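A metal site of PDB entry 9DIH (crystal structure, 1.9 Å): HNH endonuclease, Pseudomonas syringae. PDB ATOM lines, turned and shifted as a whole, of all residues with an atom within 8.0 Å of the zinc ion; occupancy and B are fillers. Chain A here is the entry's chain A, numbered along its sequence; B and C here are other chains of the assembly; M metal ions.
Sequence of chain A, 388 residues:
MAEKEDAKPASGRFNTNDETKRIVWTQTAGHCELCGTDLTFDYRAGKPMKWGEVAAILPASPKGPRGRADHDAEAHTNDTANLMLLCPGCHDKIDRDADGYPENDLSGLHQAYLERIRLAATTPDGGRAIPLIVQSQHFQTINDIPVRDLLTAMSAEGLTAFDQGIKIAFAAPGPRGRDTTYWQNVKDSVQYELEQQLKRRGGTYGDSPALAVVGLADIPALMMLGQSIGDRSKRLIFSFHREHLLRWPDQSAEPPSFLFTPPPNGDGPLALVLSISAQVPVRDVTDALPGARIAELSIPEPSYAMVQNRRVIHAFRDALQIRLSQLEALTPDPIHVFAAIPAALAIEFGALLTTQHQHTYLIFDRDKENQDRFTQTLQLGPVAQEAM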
ATOM      1  N   HIS A  31      12.836  20.290 -11.199  1.00  0.00           N
ATOM      2  CA  HIS A  31      13.424  20.701  -9.944  1.00  0.00           C
ATOM      3  C   HIS A  31      12.349  21.294  -9.022  1.00  0.00           C
ATOM      4  O   HIS A  31      11.304  21.773  -9.466  1.00  0.00           O
ATOM      5  CB  HIS A  31      14.535  21.788 -10.177  1.00  0.00           C
ATOM      6  CG  HIS A  31      15.786  21.275 -10.842  1.00  0.00           C
ATOM      7  ND1 HIS A  31      15.805  20.649 -12.056  1.00  0.00           N
ATOM      8  CD2 HIS A  31      17.085  21.317 -10.432  1.00  0.00           C
ATOM      9  CE1 HIS A  31      17.050  20.343 -12.397  1.00  0.00           C
ATOM     10  NE2 HIS A  31      17.850  20.732 -11.427  1.00  0.00           N
ATOM     11  N   CYS A  32      12.612  21.212  -7.740  1.00  0.00           N
ATOM     12  CA  CYS A  32      11.699  21.668  -6.684  1.00  0.00           C
ATOM     13  C   CYS A  32      11.620  23.156  -6.691  1.00  0.00           C
ATOM     14  O   CYS A  32      12.643  23.823  -6.594  1.00  0.00           O
ATOM     15  CB  CYS A  32      12.187  21.211  -5.355  1.00  0.00           C
ATOM     16  SG  CYS A  32      11.179  21.767  -3.993  1.00  0.00           S
ATOM     17  N   GLU A  33      10.412  23.687  -6.829  1.00  0.00           N
ATOM     18  CA  GLU A  33      10.275  25.143  -7.029  1.00  0.00           C
ATOM     19  C   GLU A  33      10.665  25.898  -5.826  1.00  0.00           C
ATOM     20  O   GLU A  33      10.888  27.127  -5.921  1.00  0.00           O
ATOM     21  CB  GLU A  33       8.822  25.489  -7.420  1.00  0.00           C
ATOM     22  CG  GLU A  33       8.319  24.757  -8.683  1.00  0.00           C
ATOM     23  CD  GLU A  33       7.037  25.360  -9.224  1.00  0.00           C
ATOM     24  OE1 GLU A  33       6.905  26.583  -9.103  1.00  0.00           O
ATOM     25  OE2 GLU A  33       6.169  24.617  -9.788  1.00  0.00           O
ATOM     26  N   LEU A  34      10.722  25.236  -4.651  1.00  0.00           N
ATOM     27  CA  LEU A  34      11.049  25.916  -3.407  1.00  0.00           C
ATOM     28  C   LEU A  34      12.474  25.703  -2.928  1.00  0.00           C
ATOM     29  O   LEU A  34      12.930  26.566  -2.172  1.00  0.00           O
ATOM     30  CB  LEU A  34      10.091  25.489  -2.262  1.00  0.00           C
ATOM     31  CG  LEU A  34       8.657  25.980  -2.483  1.00  0.00           C
ATOM     32  CD1 LEU A  34       7.712  25.431  -1.469  1.00  0.00           C
ATOM     33  CD2 LEU A  34       8.635  27.546  -2.382  1.00  0.00           C
ATOM     34  N   CYS A  35      13.189  24.613  -3.321  1.00  0.00           N
ATOM     35  CA  CYS A  35      14.594  24.415  -2.824  1.00  0.00           C
ATOM     36  C   CYS A  35      15.592  24.159  -3.930  1.00  0.00           C
ATOM     37  O   CYS A  35      16.760  24.238  -3.674  1.00  0.00           O
ATOM     38  CB  CYS A  35      14.710  23.273  -1.817  1.00  0.00           C
ATOM     39  SG  CYS A  35      14.552  21.603  -2.446  1.00  0.00           S
ATOM     40  N   GLY A  36      15.166  23.910  -5.137  1.00  0.00           N
ATOM     41  CA  GLY A  36      15.979  23.787  -6.297  1.00  0.00           C
ATOM     42  C   GLY A  36      16.572  22.434  -6.527  1.00  0.00           C
ATOM     43  O   GLY A  36      17.395  22.303  -7.424  1.00  0.00           O
ATOM     44  N   THR A  37      16.266  21.452  -5.713  1.00  0.00           N
ATOM     45  CA  THR A  37      16.896  20.151  -5.864  1.00  0.00           C
ATOM     46  C   THR A  37      16.395  19.500  -7.133  1.00  0.00           C
ATOM     47  O   THR A  37      15.268  19.687  -7.549  1.00  0.00           O
ATOM     48  CB  THR A  37      16.643  19.322  -4.587  1.00  0.00           C
ATOM     49  OG1 THR A  37      17.484  18.191  -4.556  1.00  0.00           O
ATOM     50  CG2 THR A  37      15.241  18.802  -4.602  1.00  0.00           C
ATOM     51  N   ASP A  38      17.272  18.711  -7.751  1.00  0.00           N
ATOM     52  CA  ASP A  38      16.949  17.936  -8.948  1.00  0.00           C
ATOM     53  C   ASP A  38      16.106  16.726  -8.565  1.00  0.00           C
ATOM     54  O   ASP A  38      16.541  15.828  -7.818  1.00  0.00           O
ATOM     55  CB  ASP A  38      18.232  17.451  -9.623  1.00  0.00           C
ATOM     56  CG  ASP A  38      17.987  16.771 -10.952  1.00  0.00           C
ATOM     57  OD1 ASP A  38      16.831  16.443 -11.338  1.00  0.00           O
ATOM     58  OD2 ASP A  38      18.991  16.546 -11.638  1.00  0.00           O
ATOM     59  N   LEU A  39      14.949  16.661  -9.144  1.00  0.00           N
ATOM     60  CA  LEU A  39      13.972  15.636  -8.807  1.00  0.00           C
ATOM     61  C   LEU A  39      13.834  14.599  -9.878  1.00  0.00           C
ATOM     62  O   LEU A  39      12.851  13.852  -9.865  1.00  0.00           O
ATOM     63  CB  LEU A  39      12.605  16.298  -8.564  1.00  0.00           C
ATOM     64  CG  LEU A  39      12.543  17.169  -7.312  1.00  0.00           C
ATOM     65  CD1 LEU A  39      11.302  17.968  -7.354  1.00  0.00           C
ATOM     66  CD2 LEU A  39      12.605  16.326  -6.042  1.00  0.00           C
ATOM     67  N   TRP A  51      11.146  11.639  -8.335  1.00  0.00           N
ATOM     68  CA  TRP A  51      10.844  11.520  -6.918  1.00  0.00           C
ATOM     69  C   TRP A  51      10.209  12.788  -6.352  1.00  0.00           C
ATOM     70  O   TRP A  51      10.143  12.957  -5.124  1.00  0.00           O
ATOM     71  CB  TRP A  51      12.089  11.139  -6.085  1.00  0.00           C
ATOM     72  CG  TRP A  51      13.237  12.025  -6.158  1.00  0.00           C
ATOM     73  CD1 TRP A  51      14.154  12.103  -7.156  1.00  0.00           C
ATOM     74  CD2 TRP A  51      13.718  12.935  -5.113  1.00  0.00           C
ATOM     75  NE1 TRP A  51      15.161  13.019  -6.819  1.00  0.00           N
ATOM     76  CE2 TRP A  51      14.884  13.555  -5.585  1.00  0.00           C
ATOM     77  CE3 TRP A  51      13.275  13.271  -3.844  1.00  0.00           C
ATOM     78  CZ2 TRP A  51      15.599  14.488  -4.837  1.00  0.00           C
ATOM     79  CZ3 TRP A  51      13.946  14.223  -3.120  1.00  0.00           C
ATOM     80  CH2 TRP A  51      15.088  14.827  -3.613  1.00  0.00           C
ATOM     81  N   LEU A  85       5.730  21.831  -8.645  1.00  0.00           N
ATOM     82  CA  LEU A  85       6.545  20.636  -8.459  1.00  0.00           C
ATOM     83  C   LEU A  85       7.390  20.866  -7.202  1.00  0.00           C
ATOM     84  O   LEU A  85       8.188  21.805  -7.163  1.00  0.00           O
ATOM     85  CB  LEU A  85       7.464  20.384  -9.652  1.00  0.00           C
ATOM     86  CG  LEU A  85       8.175  19.051  -9.583  1.00  0.00           C
ATOM     87  CD1 LEU A  85       7.107  17.904  -9.765  1.00  0.00           C
ATOM     88  CD2 LEU A  85       9.206  18.985 -10.682  1.00  0.00           C
ATOM     89  N   LEU A  86       7.214  20.033  -6.211  1.00  0.00           N
ATOM     90  CA  LEU A  86       7.959  20.152  -4.951  1.00  0.00           C
ATOM     91  C   LEU A  86       8.606  18.820  -4.585  1.00  0.00           C
ATOM     92  O   LEU A  86       8.086  17.737  -4.885  1.00  0.00           O
ATOM     93  CB  LEU A  86       7.030  20.531  -3.800  1.00  0.00           C
ATOM     94  CG  LEU A  86       6.290  21.881  -3.983  1.00  0.00           C
ATOM     95  CD1 LEU A  86       5.390  21.997  -2.868  1.00  0.00           C
ATOM     96  CD2 LEU A  86       7.274  23.046  -4.039  1.00  0.00           C
ATOM     97  N   CYS A  87       9.729  18.900  -3.920  1.00  0.00           N
ATOM     98  CA  CYS A  87      10.275  17.679  -3.319  1.00  0.00           C
ATOM     99  C   CYS A  87       9.357  17.262  -2.182  1.00  0.00           C
ATOM    100  O   CYS A  87       8.598  18.069  -1.658  1.00  0.00           O
ATOM    101  CB  CYS A  87      11.704  17.894  -2.814  1.00  0.00           C
ATOM    102  SG  CYS A  87      11.871  18.949  -1.441  1.00  0.00           S
ATOM    103  N   PRO A  88       9.390  15.989  -1.794  1.00  0.00           N
ATOM    104  CA  PRO A  88       8.461  15.554  -0.757  1.00  0.00           C
ATOM    105  C   PRO A  88       8.637  16.278   0.584  1.00  0.00           C
ATOM    106  O   PRO A  88       7.651  16.443   1.346  1.00  0.00           O
ATOM    107  CB  PRO A  88       8.703  14.037  -0.676  1.00  0.00           C
ATOM    108  CG  PRO A  88       9.341  13.656  -1.968  1.00  0.00           C
ATOM    109  CD  PRO A  88      10.114  14.875  -2.436  1.00  0.00           C
ATOM    110  N   GLY A  89       9.846  16.698   0.926  1.00  0.00           N
ATOM    111  CA  GLY A  89      10.024  17.401   2.168  1.00  0.00           C
ATOM    112  C   GLY A  89       9.429  18.791   2.143  1.00  0.00           C
ATOM    113  O   GLY A  89       8.693  19.179   3.076  1.00  0.00           O
ATOM    114  N   CYS A  90       9.743  19.581   1.125  1.00  0.00           N
ATOM    115  CA  CYS A  90       9.089  20.897   0.941  1.00  0.00           C
ATOM    116  C   CYS A  90       7.576  20.751   0.917  1.00  0.00           C
ATOM    117  O   CYS A  90       6.876  21.483   1.593  1.00  0.00           O
ATOM    118  CB  CYS A  90       9.589  21.526  -0.353  1.00  0.00           C
ATOM    119  SG  CYS A  90      11.365  22.058  -0.111  1.00  0.00           S
ATOM    120  N   HIS A  91       7.067  19.772   0.187  1.00  0.00           N
ATOM    121  CA  HIS A  91       5.622  19.605   0.160  1.00  0.00           C
ATOM    122  C   HIS A  91       5.067  19.263   1.527  1.00  0.00           C
ATOM    123  O   HIS A  91       4.018  19.772   1.915  1.00  0.00           O
ATOM    124  CB  HIS A  91       5.263  18.491  -0.840  1.00  0.00           C
ATOM    125  CG  HIS A  91       3.785  18.350  -1.073  1.00  0.00           C
ATOM    126  ND1 HIS A  91       3.231  17.193  -1.560  1.00  0.00           N
ATOM    127  CD2 HIS A  91       2.767  19.233  -0.945  1.00  0.00           C
ATOM    128  CE1 HIS A  91       1.916  17.357  -1.695  1.00  0.00           C
ATOM    129  NE2 HIS A  91       1.616  18.606  -1.366  1.00  0.00           N
ATOM    130  N   LYS A  93       6.296  20.110   4.481  1.00  0.00           N
ATOM    131  CA  LYS A  93       6.345  21.301   5.332  1.00  0.00           C
ATOM    132  C   LYS A  93       5.238  22.307   4.981  1.00  0.00           C
ATOM    133  O   LYS A  93       4.554  22.832   5.866  1.00  0.00           O
ATOM    134  CB  LYS A  93       7.723  21.974   5.212  1.00  0.00           C
ATOM    135  CG  LYS A  93       8.890  21.199   5.881  1.00  0.00           C
ATOM    136  CD  LYS A  93      10.209  21.547   5.220  1.00  0.00           C
ATOM    137  CE  LYS A  93      11.393  20.829   5.815  1.00  0.00           C
ATOM    138  NZ  LYS A  93      12.675  21.426   5.302  1.00  0.00           N
ATOM    139  N   ARG B  44      12.839  27.000   7.774  1.00  0.00           N
ATOM    140  CA  ARG B  44      12.573  28.018   6.787  1.00  0.00           C
ATOM    141  C   ARG B  44      11.536  29.003   7.287  1.00  0.00           C
ATOM    142  O   ARG B  44      11.635  30.215   7.034  1.00  0.00           O
ATOM    143  CB  ARG B  44      12.132  27.404   5.468  1.00  0.00           C
ATOM    144  CG  ARG B  44      11.516  28.373   4.501  1.00  0.00           C
ATOM    145  CD  ARG B  44      11.404  27.874   3.035  1.00  0.00           C
ATOM    146  NE  ARG B  44      10.811  28.861   2.118  1.00  0.00           N
ATOM    147  CZ  ARG B  44      11.084  28.922   0.825  1.00  0.00           C
ATOM    148  NH1 ARG B  44      11.764  27.950   0.238  1.00  0.00           N
ATOM    149  NH2 ARG B  44      10.625  29.947   0.105  1.00  0.00           N
ATOM    150  N   PRO C 124      16.512  28.563  -6.611  1.00  0.00           N
ATOM    151  CA  PRO C 124      16.061  28.593  -5.186  1.00  0.00           C
ATOM    152  C   PRO C 124      17.134  28.288  -4.181  1.00  0.00           C
ATOM    153  O   PRO C 124      17.049  28.854  -3.077  1.00  0.00           O
ATOM    154  CB  PRO C 124      14.981  27.542  -5.176  1.00  0.00           C
ATOM    155  CG  PRO C 124      14.366  27.688  -6.528  1.00  0.00           C
ATOM    156  CD  PRO C 124      15.550  27.899  -7.438  1.00  0.00           C
HETATM  157 ZN    ZN M   1      12.298  21.186  -2.057  1.00  0.00          ZN
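The backbone carbonyl oxygen (O) of Thr 37 sits at hydrogen-bond distance from the backbone NH (N) of Cys 32, at 3.1 Å.
The side-chain sulfur of Cys 32 sits close to the backbone NH of Leu 34, 3.6 Å away.
The backbone NH (N) of Thr 37 lies close to the side-chain sulfur (SG) of Cys 35 (3.7 Å).
Four residues have an atom within 4 Å of the zinc ion: Cys 32, Cys 35, Cys 87 and Cys 90.
The nearest printed residue that does not touch the zinc ion is Thr 37 (4.6 Å).
The zinc ion is bound by the side-chain sulfur (SG) of Cys 32 (2.3 Å), the side-chain sulfur (SG) of Cys 35 (2.3 Å), the side-chain sulfur (SG) of Cys 90 (2.3 Å) and the side-chain sulfur (SG) of Cys 87 (2.4 Å).
The zinc ion has four donor atoms within binding distance.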
